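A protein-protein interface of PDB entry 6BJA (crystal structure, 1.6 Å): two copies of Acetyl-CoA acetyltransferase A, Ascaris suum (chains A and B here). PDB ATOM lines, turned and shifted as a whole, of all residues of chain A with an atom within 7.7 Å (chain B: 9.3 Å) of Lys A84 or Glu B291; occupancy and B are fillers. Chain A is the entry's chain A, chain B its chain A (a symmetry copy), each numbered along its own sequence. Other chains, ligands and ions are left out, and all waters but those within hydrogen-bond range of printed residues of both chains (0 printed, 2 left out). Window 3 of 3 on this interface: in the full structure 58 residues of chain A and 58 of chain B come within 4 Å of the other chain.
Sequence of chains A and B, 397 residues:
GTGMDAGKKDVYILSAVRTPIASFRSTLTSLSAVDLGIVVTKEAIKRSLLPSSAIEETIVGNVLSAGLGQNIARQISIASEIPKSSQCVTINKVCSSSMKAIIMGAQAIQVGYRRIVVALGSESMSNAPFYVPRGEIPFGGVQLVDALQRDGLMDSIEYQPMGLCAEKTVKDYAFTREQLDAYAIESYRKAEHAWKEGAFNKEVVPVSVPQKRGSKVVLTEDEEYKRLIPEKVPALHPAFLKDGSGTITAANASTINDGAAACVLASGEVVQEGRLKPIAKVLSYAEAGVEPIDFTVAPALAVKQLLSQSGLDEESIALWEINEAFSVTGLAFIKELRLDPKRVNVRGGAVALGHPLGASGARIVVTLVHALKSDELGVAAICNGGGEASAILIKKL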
ATOM      1  N   ILE A  55      22.226   5.937  23.776  1.00  0.00           N
ATOM      2  CA  ILE A  55      22.910   4.697  23.411  1.00  0.00           C
ATOM      3  C   ILE A  55      23.649   4.890  22.092  1.00  0.00           C
ATOM      4  O   ILE A  55      23.021   5.195  21.079  1.00  0.00           O
ATOM      5  CB  ILE A  55      21.924   3.531  23.273  1.00  0.00           C
ATOM      6  CG1 ILE A  55      21.038   3.385  24.520  1.00  0.00           C
ATOM      7  CG2 ILE A  55      22.699   2.238  22.973  1.00  0.00           C
ATOM      8  CD1 ILE A  55      21.791   3.167  25.829  1.00  0.00           C
ATOM      9  N   ARG A  74      20.948  -4.005  13.908  1.00  0.00           N
ATOM     10  CA  ARG A  74      20.347  -2.754  13.445  1.00  0.00           C
ATOM     11  C   ARG A  74      18.811  -2.781  13.561  1.00  0.00           C
ATOM     12  O   ARG A  74      18.183  -1.781  13.911  1.00  0.00           O
ATOM     13  CB  ARG A  74      20.772  -2.487  12.014  1.00  0.00           C
ATOM     14  CG  ARG A  74      20.273  -1.165  11.443  1.00  0.00           C
ATOM     15  CD  ARG A  74      20.929   0.016  12.108  1.00  0.00           C
ATOM     16  NE  ARG A  74      20.701   1.250  11.322  1.00  0.00           N
ATOM     17  CZ  ARG A  74      21.045   2.466  11.730  1.00  0.00           C
ATOM     18  NH1 ARG A  74      21.681   2.648  12.881  1.00  0.00           N
ATOM     19  NH2 ARG A  74      20.776   3.516  10.959  1.00  0.00           N
ATOM     20  N   SER A  77      18.101  -2.316  17.251  1.00  0.00           N
ATOM     21  CA  SER A  77      18.421  -0.968  17.677  1.00  0.00           C
ATOM     22  C   SER A  77      17.325   0.014  17.256  1.00  0.00           C
ATOM     23  O   SER A  77      16.805   0.791  18.071  1.00  0.00           O
ATOM     24  CB  SER A  77      19.762  -0.570  17.088  1.00  0.00           C
ATOM     25  OG  SER A  77      20.244   0.665  17.557  1.00  0.00           O
ATOM     26  N   ILE A  78      16.962  -0.036  15.985  1.00  0.00           N
ATOM     27  CA  ILE A  78      15.943   0.890  15.476  1.00  0.00           C
ATOM     28  C   ILE A  78      14.602   0.674  16.177  1.00  0.00           C
ATOM     29  O   ILE A  78      13.926   1.653  16.591  1.00  0.00           O
ATOM     30  CB  ILE A  78      15.791   0.754  13.948  1.00  0.00           C
ATOM     31  CG1 ILE A  78      17.004   1.387  13.276  1.00  0.00           C
ATOM     32  CG2 ILE A  78      14.492   1.431  13.459  1.00  0.00           C
ATOM     33  CD1 ILE A  78      17.046   1.220  11.770  1.00  0.00           C
ATOM     34  N   ALA A  79      14.205  -0.588  16.348  1.00  0.00           N
ATOM     35  CA  ALA A  79      12.919  -0.904  16.975  1.00  0.00           C
ATOM     36  C   ALA A  79      12.904  -0.600  18.474  1.00  0.00           C
ATOM     37  O   ALA A  79      11.819  -0.458  19.076  1.00  0.00           O
ATOM     38  CB  ALA A  79      12.558  -2.344  16.738  1.00  0.00           C
ATOM     39  N   GLU A  81      14.102   2.239  19.584  1.00  0.00           N
ATOM     40  CA  GLU A  81      14.166   3.708  19.599  1.00  0.00           C
ATOM     41  C   GLU A  81      15.556   4.282  19.878  1.00  0.00           C
ATOM     42  O   GLU A  81      15.713   5.391  20.364  1.00  0.00           O
ATOM     43  CB  GLU A  81      13.144   4.238  20.611  1.00  0.00           C
ATOM     44  CG  GLU A  81      11.727   3.799  20.252  1.00  0.00           C
ATOM     45  CD  GLU A  81      10.654   4.442  21.125  1.00  0.00           C
ATOM     46  OE1 GLU A  81      10.901   4.654  22.333  1.00  0.00           O
ATOM     47  OE2 GLU A  81       9.561   4.740  20.595  1.00  0.00           O
ATOM     48  N   ILE A  82      16.591   3.511  19.559  1.00  0.00           N
ATOM     49  CA  ILE A  82      17.954   4.013  19.589  1.00  0.00           C
ATOM     50  C   ILE A  82      18.162   4.834  18.306  1.00  0.00           C
ATOM     51  O   ILE A  82      17.627   4.461  17.277  1.00  0.00           O
ATOM     52  CB  ILE A  82      18.937   2.841  19.719  1.00  0.00           C
ATOM     53  CG1 ILE A  82      18.744   2.188  21.086  1.00  0.00           C
ATOM     54  CG2 ILE A  82      20.378   3.288  19.575  1.00  0.00           C
ATOM     55  CD1 ILE A  82      19.513   0.873  21.241  1.00  0.00           C
ATOM     56  N   PRO A  83      18.920   5.944  18.381  1.00  0.00           N
ATOM     57  CA  PRO A  83      19.022   6.839  17.216  1.00  0.00           C
ATOM     58  C   PRO A  83      19.562   6.146  15.985  1.00  0.00           C
ATOM     59  O   PRO A  83      20.399   5.239  16.084  1.00  0.00           O
ATOM     60  CB  PRO A  83      20.005   7.907  17.682  1.00  0.00           C
ATOM     61  CG  PRO A  83      19.831   7.954  19.153  1.00  0.00           C
ATOM     62  CD  PRO A  83      19.618   6.516  19.549  1.00  0.00           C
ATOM     63  N   LYS A  84      19.104   6.593  14.828  1.00  0.00           N
ATOM     64  CA  LYS A  84      19.631   6.088  13.563  1.00  0.00           C
ATOM     65  C   LYS A  84      21.125   6.324  13.438  1.00  0.00           C
ATOM     66  O   LYS A  84      21.789   5.595  12.709  1.00  0.00           O
ATOM     67  CB  LYS A  84      18.922   6.727  12.386  1.00  0.00           C
ATOM     68  CG  LYS A  84      17.436   6.549  12.338  1.00  0.00           C
ATOM     69  CD  LYS A  84      16.979   5.126  12.183  1.00  0.00           C
ATOM     70  CE  LYS A  84      15.431   5.018  12.193  1.00  0.00           C
ATOM     71  NZ  LYS A  84      14.732   5.616  13.369  1.00  0.00           N
ATOM     72  N   SER A  85      21.654   7.322  14.138  1.00  0.00           N
ATOM     73  CA  SER A  85      23.078   7.618  14.103  1.00  0.00           C
ATOM     74  C   SER A  85      23.944   6.613  14.867  1.00  0.00           C
ATOM     75  O   SER A  85      25.156   6.614  14.718  1.00  0.00           O
ATOM     76  CB  SER A  85      23.348   9.022  14.651  1.00  0.00           C
ATOM     77  OG  SER A  85      22.826   9.178  15.955  1.00  0.00           O
ATOM     78  N   SER A  86      23.327   5.753  15.663  1.00  0.00           N
ATOM     79  CA  SER A  86      24.079   4.809  16.466  1.00  0.00           C
ATOM     80  C   SER A  86      24.489   3.611  15.632  1.00  0.00           C
ATOM     81  O   SER A  86      23.775   3.202  14.720  1.00  0.00           O
ATOM     82  CB  SER A  86      23.256   4.378  17.676  1.00  0.00           C
ATOM     83  OG  SER A  86      23.003   5.512  18.482  1.00  0.00           O
ATOM     84  N   GLN A  87      25.650   3.055  15.954  1.00  0.00           N
ATOM     85  CA  GLN A  87      26.240   1.963  15.200  1.00  0.00           C
ATOM     86  C   GLN A  87      25.825   0.588  15.707  1.00  0.00           C
ATOM     87  O   GLN A  87      25.812   0.353  16.906  1.00  0.00           O
ATOM     88  CB  GLN A  87      27.742   2.077  15.262  1.00  0.00           C
ATOM     89  CG  GLN A  87      28.351   3.031  14.246  1.00  0.00           C
ATOM     90  CD  GLN A  87      27.766   4.429  14.282  1.00  0.00           C
ATOM     91  OE1 GLN A  87      28.093   5.226  15.179  1.00  0.00           O
ATOM     92  NE2 GLN A  87      26.903   4.754  13.294  1.00  0.00           N
ATOM     93  N   CYS A  88      25.535  -0.308  14.773  1.00  0.00           N
ATOM     94  CA  CYS A  88      24.978  -1.627  15.071  1.00  0.00           C
ATOM     95  C   CYS A  88      25.720  -2.748  14.372  1.00  0.00           C
ATOM     96  O   CYS A  88      25.926  -2.684  13.173  1.00  0.00           O
ATOM     97  CB  CYS A  88      23.531  -1.665  14.643  1.00  0.00           C
ATOM     98  SG  CYS A  88      22.568  -0.298  15.360  1.00  0.00           S
ATOM     99  N   LYS B  93      27.952  -6.605   9.380  1.00  0.00           N
ATOM    100  CA  LYS B  93      27.408  -5.265   9.253  1.00  0.00           C
ATOM    101  C   LYS B  93      27.020  -5.062   7.780  1.00  0.00           C
ATOM    102  O   LYS B  93      27.273  -4.000   7.166  1.00  0.00           O
ATOM    103  CB  LYS B  93      28.411  -4.224   9.740  1.00  0.00           C
ATOM    104  CG  LYS B  93      27.805  -2.866  10.112  1.00  0.00           C
ATOM    105  CD  LYS B  93      28.870  -2.022  10.768  1.00  0.00           C
ATOM    106  CE  LYS B  93      28.439  -0.606  10.951  1.00  0.00           C
ATOM    107  NZ  LYS B  93      27.648  -0.463  12.159  1.00  0.00           N
ATOM    108  N   ASP B 155      16.288  -4.536   2.383  1.00  0.00           N
ATOM    109  CA  ASP B 155      16.344  -3.838   3.647  1.00  0.00           C
ATOM    110  C   ASP B 155      15.278  -4.419   4.548  1.00  0.00           C
ATOM    111  O   ASP B 155      14.126  -4.545   4.139  1.00  0.00           O
ATOM    112  CB  ASP B 155      16.122  -2.340   3.475  1.00  0.00           C
ATOM    113  CG  ASP B 155      16.209  -1.620   4.798  1.00  0.00           C
ATOM    114  OD1 ASP B 155      15.209  -1.609   5.536  1.00  0.00           O
ATOM    115  OD2 ASP B 155      17.301  -1.113   5.126  1.00  0.00           O
ATOM    116  N   ILE B 157      14.099  -3.267   7.415  1.00  0.00           N
ATOM    117  CA  ILE B 157      13.299  -2.317   8.173  1.00  0.00           C
ATOM    118  C   ILE B 157      12.223  -1.750   7.262  1.00  0.00           C
ATOM    119  O   ILE B 157      11.062  -1.637   7.674  1.00  0.00           O
ATOM    120  CB  ILE B 157      14.182  -1.208   8.788  1.00  0.00           C
ATOM    121  CG1 ILE B 157      14.974  -1.788   9.967  1.00  0.00           C
ATOM    122  CG2 ILE B 157      13.352  -0.037   9.285  1.00  0.00           C
ATOM    123  CD1 ILE B 157      16.418  -1.816   9.789  1.00  0.00           C
ATOM    124  N   GLU B 158      12.604  -1.408   6.024  1.00  0.00           N
ATOM    125  CA  GLU B 158      11.678  -0.929   5.005  1.00  0.00           C
ATOM    126  C   GLU B 158      10.995  -2.064   4.238  1.00  0.00           C
ATOM    127  O   GLU B 158      10.013  -1.850   3.531  1.00  0.00           O
ATOM    128  CB  GLU B 158      12.423  -0.022   4.013  1.00  0.00           C
ATOM    129  CG  GLU B 158      12.920   1.285   4.618  1.00  0.00           C
ATOM    130  CD  GLU B 158      11.823   2.330   4.772  1.00  0.00           C
ATOM    131  OE1 GLU B 158      10.691   2.098   4.289  1.00  0.00           O
ATOM    132  OE2 GLU B 158      12.099   3.386   5.376  1.00  0.00           O
ATOM    133  N   CYS B 165      15.220   1.565  -2.329  1.00  0.00           N
ATOM    134  CA  CYS B 165      15.624   2.614  -1.407  1.00  0.00           C
ATOM    135  C   CYS B 165      16.519   3.646  -2.092  1.00  0.00           C
ATOM    136  O   CYS B 165      16.378   4.844  -1.902  1.00  0.00           O
ATOM    137  CB  CYS B 165      16.364   2.020  -0.213  1.00  0.00           C
ATOM    138  SG  CYS B 165      15.326   0.941   0.855  1.00  0.00           S
ATOM    139  N   LYS B 168      15.270   6.760  -3.880  1.00  0.00           N
ATOM    140  CA  LYS B 168      14.967   7.979  -3.139  1.00  0.00           C
ATOM    141  C   LYS B 168      16.126   8.980  -3.246  1.00  0.00           C
ATOM    142  O   LYS B 168      15.921  10.192  -3.443  1.00  0.00           O
ATOM    143  CB  LYS B 168      14.653   7.670  -1.660  1.00  0.00           C
ATOM    144  CG  LYS B 168      14.423   8.940  -0.831  1.00  0.00           C
ATOM    145  CD  LYS B 168      14.026   8.646   0.586  1.00  0.00           C
ATOM    146  CE  LYS B 168      13.726   9.935   1.350  1.00  0.00           C
ATOM    147  NZ  LYS B 168      14.879  10.874   1.428  1.00  0.00           N
ATOM    148  N   THR B 169      17.347   8.473  -3.169  1.00  0.00           N
ATOM    149  CA  THR B 169      18.535   9.314  -3.194  1.00  0.00           C
ATOM    150  C   THR B 169      18.692   9.870  -4.608  1.00  0.00           C
ATOM    151  O   THR B 169      19.071  11.025  -4.787  1.00  0.00           O
ATOM    152  CB  THR B 169      19.772   8.526  -2.737  1.00  0.00           C
ATOM    153  OG1 THR B 169      19.517   8.040  -1.399  1.00  0.00           O
ATOM    154  CG2 THR B 169      21.028   9.411  -2.760  1.00  0.00           C
ATOM    155  N   GLU B 287      32.232   6.476  11.665  1.00  0.00           N
ATOM    156  CA  GLU B 287      31.042   5.716  11.357  1.00  0.00           C
ATOM    157  C   GLU B 287      29.859   6.661  11.457  1.00  0.00           C
ATOM    158  O   GLU B 287      29.836   7.516  12.335  1.00  0.00           O
ATOM    159  CB  GLU B 287      30.876   4.547  12.322  1.00  0.00           C
ATOM    160  CG  GLU B 287      32.073   3.582  12.344  1.00  0.00           C
ATOM    161  CD  GLU B 287      32.008   2.560  13.475  1.00  0.00           C
ATOM    162  OE1 GLU B 287      32.011   2.969  14.654  1.00  0.00           O
ATOM    163  OE2 GLU B 287      31.989   1.348  13.189  1.00  0.00           O
ATOM    164  N   ALA B 288      28.910   6.510  10.548  1.00  0.00           N
ATOM    165  CA  ALA B 288      27.714   7.340  10.523  1.00  0.00           C
ATOM    166  C   ALA B 288      26.472   6.495  10.339  1.00  0.00           C
ATOM    167  O   ALA B 288      26.528   5.355   9.864  1.00  0.00           O
ATOM    168  CB  ALA B 288      27.812   8.359   9.415  1.00  0.00           C
ATOM    169  N   GLY B 289      25.337   7.043  10.744  1.00  0.00           N
ATOM    170  CA  GLY B 289      24.084   6.370  10.506  1.00  0.00           C
ATOM    171  C   GLY B 289      22.948   7.332  10.213  1.00  0.00           C
ATOM    172  O   GLY B 289      22.857   8.409  10.807  1.00  0.00           O
ATOM    173  N   VAL B 290      22.070   6.896   9.317  1.00  0.00           N
ATOM    174  CA  VAL B 290      20.893   7.654   8.907  1.00  0.00           C
ATOM    175  C   VAL B 290      19.683   6.723   8.792  1.00  0.00           C
ATOM    176  O   VAL B 290      19.758   5.532   9.118  1.00  0.00           O
ATOM    177  CB  VAL B 290      21.147   8.359   7.555  1.00  0.00           C
ATOM    178  CG1 VAL B 290      22.327   9.314   7.651  1.00  0.00           C
ATOM    179  CG2 VAL B 290      21.403   7.338   6.495  1.00  0.00           C
ATOM    180  N   GLU B 291      18.548   7.247   8.350  1.00  0.00           N
ATOM    181  CA  GLU B 291      17.393   6.409   8.055  1.00  0.00           C
ATOM    182  C   GLU B 291      17.758   5.291   7.082  1.00  0.00           C
ATOM    183  O   GLU B 291      18.486   5.526   6.119  1.00  0.00           O
ATOM    184  CB  GLU B 291      16.266   7.255   7.452  1.00  0.00           C
ATOM    185  CG  GLU B 291      15.656   8.236   8.432  1.00  0.00           C
ATOM    186  CD  GLU B 291      14.744   7.572   9.444  1.00  0.00           C
ATOM    187  OE1 GLU B 291      14.227   6.470   9.174  1.00  0.00           O
ATOM    188  OE2 GLU B 291      14.537   8.166  10.513  1.00  0.00           O
ATOM    189  N   PRO B 292      17.232   4.080   7.299  1.00  0.00           N
ATOM    190  CA  PRO B 292      17.534   2.983   6.368  1.00  0.00           C
ATOM    191  C   PRO B 292      17.339   3.340   4.892  1.00  0.00           C
ATOM    192  O   PRO B 292      18.185   2.993   4.071  1.00  0.00           O
ATOM    193  CB  PRO B 292      16.566   1.891   6.828  1.00  0.00           C
ATOM    194  CG  PRO B 292      16.571   2.079   8.305  1.00  0.00           C
ATOM    195  CD  PRO B 292      16.574   3.569   8.524  1.00  0.00           C
ATOM    196  N   ILE B 293      16.250   4.026   4.559  1.00  0.00           N
ATOM    197  CA  ILE B 293      15.975   4.312   3.159  1.00  0.00           C
ATOM    198  C   ILE B 293      17.060   5.213   2.566  1.00  0.00           C
ATOM    199  O   ILE B 293      17.294   5.183   1.357  1.00  0.00           O
ATOM    200  CB  ILE B 293      14.571   4.952   2.997  1.00  0.00           C
ATOM    201  CG1 ILE B 293      14.152   4.905   1.523  1.00  0.00           C
ATOM    202  CG2 ILE B 293      14.543   6.353   3.551  1.00  0.00           C
ATOM    203  CD1 ILE B 293      12.658   5.142   1.314  1.00  0.00           C
ATOM    204  N   ASP B 294      17.706   6.009   3.413  1.00  0.00           N
ATOM    205  CA  ASP B 294      18.705   6.994   2.974  1.00  0.00           C
ATOM    206  C   ASP B 294      20.147   6.482   3.062  1.00  0.00           C
ATOM    207  O   ASP B 294      21.087   7.271   3.096  1.00  0.00           O
ATOM    208  CB  ASP B 294      18.590   8.267   3.831  1.00  0.00           C
ATOM    209  CG  ASP B 294      17.299   9.040   3.577  1.00  0.00           C
ATOM    210  OD1 ASP B 294      16.927   9.196   2.394  1.00  0.00           O
ATOM    211  OD2 ASP B 294      16.648   9.493   4.569  1.00  0.00           O
ATOM    212  N   PHE B 295      20.315   5.171   3.155  1.00  0.00           N
ATOM    213  CA  PHE B 295      21.651   4.584   3.360  1.00  0.00           C
ATOM    214  C   PHE B 295      22.697   5.090   2.359  1.00  0.00           C
ATOM    215  O   PHE B 295      23.859   5.224   2.706  1.00  0.00           O
ATOM    216  CB  PHE B 295      21.584   3.050   3.311  1.00  0.00           C
ATOM    217  CG  PHE B 295      21.444   2.477   1.940  1.00  0.00           C
ATOM    218  CD1 PHE B 295      20.263   2.605   1.236  1.00  0.00           C
ATOM    219  CD2 PHE B 295      22.491   1.786   1.361  1.00  0.00           C
ATOM    220  CE1 PHE B 295      20.129   2.086  -0.033  1.00  0.00           C
ATOM    221  CE2 PHE B 295      22.360   1.253   0.109  1.00  0.00           C
ATOM    222  CZ  PHE B 295      21.189   1.405  -0.603  1.00  0.00           C
ATOM    223  N   THR B 296      22.262   5.427   1.150  1.00  0.00           N
ATOM    224  CA  THR B 296      23.172   5.853   0.110  1.00  0.00           C
ATOM    225  C   THR B 296      23.919   7.147   0.471  1.00  0.00           C
ATOM    226  O   THR B 296      25.002   7.365  -0.047  1.00  0.00           O
ATOM    227  CB  THR B 296      22.400   6.042  -1.225  1.00  0.00           C
ATOM    228  OG1 THR B 296      21.794   4.801  -1.623  1.00  0.00           O
ATOM    229  CG2 THR B 296      23.322   6.477  -2.353  1.00  0.00           C
ATOM    230  N   VAL B 297      23.355   8.020   1.320  1.00  0.00           N
ATOM    231  CA  VAL B 297      24.050   9.262   1.672  1.00  0.00           C
ATOM    232  C   VAL B 297      24.841   9.198   2.979  1.00  0.00           C
ATOM    233  O   VAL B 297      25.513  10.164   3.348  1.00  0.00           O
ATOM    234  CB  VAL B 297      23.071  10.466   1.741  1.00  0.00           C
ATOM    235  CG1 VAL B 297      22.311  10.577   0.419  1.00  0.00           C
ATOM    236  CG2 VAL B 297      22.139  10.364   2.927  1.00  0.00           C
ATOM    237  N   ALA B 298      24.823   8.052   3.656  1.00  0.00           N
ATOM    238  CA  ALA B 298      25.624   7.910   4.873  1.00  0.00           C
ATOM    239  C   ALA B 298      27.150   8.034   4.661  1.00  0.00           C
ATOM    240  O   ALA B 298      27.862   8.530   5.537  1.00  0.00           O
ATOM    241  CB  ALA B 298      25.309   6.568   5.555  1.00  0.00           C
ATOM    242  N   LEU B 301      28.470  11.501   5.094  1.00  0.00           N
ATOM    243  CA  LEU B 301      28.342  11.907   6.491  1.00  0.00           C
ATOM    244  C   LEU B 301      29.496  11.355   7.321  1.00  0.00           C
ATOM    245  O   LEU B 301      30.089  12.063   8.134  1.00  0.00           O
ATOM    246  CB  LEU B 301      26.998  11.449   7.062  1.00  0.00           C
ATOM    247  CG  LEU B 301      26.579  12.094   8.374  1.00  0.00           C
ATOM    248  CD1 LEU B 301      26.424  13.612   8.216  1.00  0.00           C
ATOM    249  CD2 LEU B 301      25.263  11.460   8.829  1.00  0.00           C
ATOM    250  N   CYS B 383      28.783   2.272   2.389  1.00  0.00           N
ATOM    251  CA  CYS B 383      27.471   2.257   3.017  1.00  0.00           C
ATOM    252  C   CYS B 383      26.980   0.831   3.192  1.00  0.00           C
ATOM    253  O   CYS B 383      27.497  -0.110   2.574  1.00  0.00           O
ATOM    254  CB  CYS B 383      26.451   3.055   2.191  1.00  0.00           C
ATOM    255  SG  CYS B 383      25.985   2.316   0.599  1.00  0.00           S
ATOM    256  N   ASN B 384      25.976   0.659   4.039  1.00  0.00           N
ATOM    257  CA  ASN B 384      25.350  -0.647   4.148  1.00  0.00           C
ATOM    258  C   ASN B 384      23.882  -0.565   4.381  1.00  0.00           C
ATOM    259  O   ASN B 384      23.375   0.415   4.915  1.00  0.00           O
ATOM    260  CB  ASN B 384      26.028  -1.523   5.230  1.00  0.00           C
ATOM    261  CG  ASN B 384      25.997  -0.941   6.634  1.00  0.00           C
ATOM    262  OD1 ASN B 384      26.978  -0.363   7.108  1.00  0.00           O
ATOM    263  ND2 ASN B 384      24.909  -1.180   7.343  1.00  0.00           N
ATOM    264  N   GLY B 385      23.194  -1.598   3.911  1.00  0.00           N
ATOM    265  CA  GLY B 385      21.782  -1.748   4.163  1.00  0.00           C
ATOM    266  C   GLY B 385      21.508  -1.562   5.641  1.00  0.00           C
ATOM    267  O   GLY B 385      22.248  -2.061   6.494  1.00  0.00           O
ATOM    268  N   GLY B 386      20.447  -0.816   5.927  1.00  0.00           N
ATOM    269  CA  GLY B 386      20.104  -0.430   7.283  1.00  0.00           C
ATOM    270  C   GLY B 386      20.407   1.013   7.616  1.00  0.00           C
ATOM    271  O   GLY B 386      19.971   1.527   8.648  1.00  0.00           O
ATOM    272  N   GLY B 387      21.158   1.683   6.754  1.00  0.00           N
ATOM    273  CA  GLY B 387      21.394   3.098   6.903  1.00  0.00           C
ATOM    274  C   GLY B 387      22.717   3.540   7.491  1.00  0.00           C
ATOM    275  O   GLY B 387      22.830   4.664   7.943  1.00  0.00           O
ATOM    276  N   GLU B 388      23.744   2.692   7.473  1.00  0.00           N
ATOM    277  CA  GLU B 388      25.000   3.065   8.098  1.00  0.00           C
ATOM    278  C   GLU B 388      26.081   3.197   7.038  1.00  0.00           C
ATOM    279  O   GLU B 388      25.904   2.777   5.889  1.00  0.00           O
ATOM    280  CB  GLU B 388      25.410   2.050   9.165  1.00  0.00           C
ATOM    281  CG  GLU B 388      24.562   2.137  10.426  1.00  0.00           C
ATOM    282  CD  GLU B 388      25.228   1.483  11.605  1.00  0.00           C
ATOM    283  OE1 GLU B 388      26.387   1.871  11.952  1.00  0.00           O
ATOM    284  OE2 GLU B 388      24.575   0.571  12.157  1.00  0.00           O
ATOM    285  N   ALA B 389      27.170   3.837   7.437  1.00  0.00           N
ATOM    286  CA  ALA B 389      28.388   3.838   6.636  1.00  0.00           C
ATOM    287  C   ALA B 389      29.618   3.936   7.516  1.00  0.00           C
ATOM    288  O   ALA B 389      29.568   4.449   8.647  1.00  0.00           O
ATOM    289  CB  ALA B 389      28.378   4.984   5.621  1.00  0.00           C
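Of the printed residues of chain B, Lys A84 touches Gly B289, Val B290, Glu B291 and Pro B292. Glu B291 touches just one residue of chain A: Lys A84 (3.6 Å). Of the printed residues of chain B, Cys A88 touches Lys B93 (3.0 Å) and Glu B388 (2.9 Å). Of the printed residues of chain A, Lys B93 touches Cys A88 (3.0 Å). Ile B293 touches none of the printed residues of chain A. The nearest printed residue of chain B that does not touch Lys A84 is Gly B387 (5.0 Å). The nearest residue of chain A that does not touch Glu B291 is Arg A74 (5.1 Å). The nearest printed residue of chain A that does not touch Glu B287 is Ser A85 (5.3 Å).
O of Ile A55 is in hydrogen-bond range of OG of Ser A86 (2.6 Å). O of Lys A84 sits at hydrogen-bond distance from NH2 of Arg A74 (2.9 Å). The backbone carbonyl oxygen (O) of Ser A86 is in hydrogen-bond range of the side-chain sulfur (SG) of Cys A88. The backbone NH (N) of Ile B157 is in hydrogen-bond range of the side-chain carboxylate (OD1) of Asp B155. O of Ala B389 sits at hydrogen-bond distance from N of Ala B288 (2.9 Å). N of Val B290 lies within hydrogen-bond range of O of Gly B387, 2.7 Å away.
NH2 of Arg A74 touches O of Gly B387, at 3.8 Å. CD1 of Ile B157 touches CD1 of Ile A78 (3.7 Å). Pro B292 touches Ile A78. Lys A84 touches Gly B289 (O to C, 3.3 Å). CB of Lys A84 touches O of Val B290 (3.6 Å). Lys A84 touches Pro B292 (CD to CD, 3.997 Å). Ser A85 touches Gly B289. OE2 of Glu B388 touches O of Ser A86 (3.8 Å). Gln A87 touches Ala B288. Gln A87 touches Gly B289 (NE2 to N, 3.8 Å).
Hydrophobic or aromatic side chains of chain B within 4 Å of the printed part of chain A: Ile B157 and Pro B292. Hydrophobic or aromatic side chains of chain A within 4 Å of the printed part of chain B: Ile A78. Along chain A the printed residues that touch a printed residue of chain B span positions 74 to 88. Among the printed residues, Asp or Glu carboxylates within 4 Å of a Lys or Arg side-chain nitrogen of the other chain: Arg A74 with Glu B388 and Lys A84 with Glu B291.
NH2 of Arg A74 lies within hydrogen-bond range of O of Val B290. The guanidinium group (NE) of Arg A74 is in hydrogen-bond range of the backbone carbonyl oxygen (O) of Gly B386. The guanidinium group (NH1) of Arg A74 lies within salt-bridge range of the side-chain carboxylate (OE2) of Glu B388 (3.6 Å). NZ of Lys A84 is in salt-bridge range of OE2 of Glu B291 (3.8 Å). The side-chain amide nitrogen (NE2) of Gln A87 lies within hydrogen-bond range of the side-chain carboxylate (OE1) of Glu B388. The backbone carbonyl oxygen (O) of Cys A88 is in hydrogen-bond range of the side-chain amino group (NZ) of Lys B93, 3.0 Å away. N of Cys A88 is in hydrogen-bond range of OE2 of Glu B388.
No position is printed for both chains.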
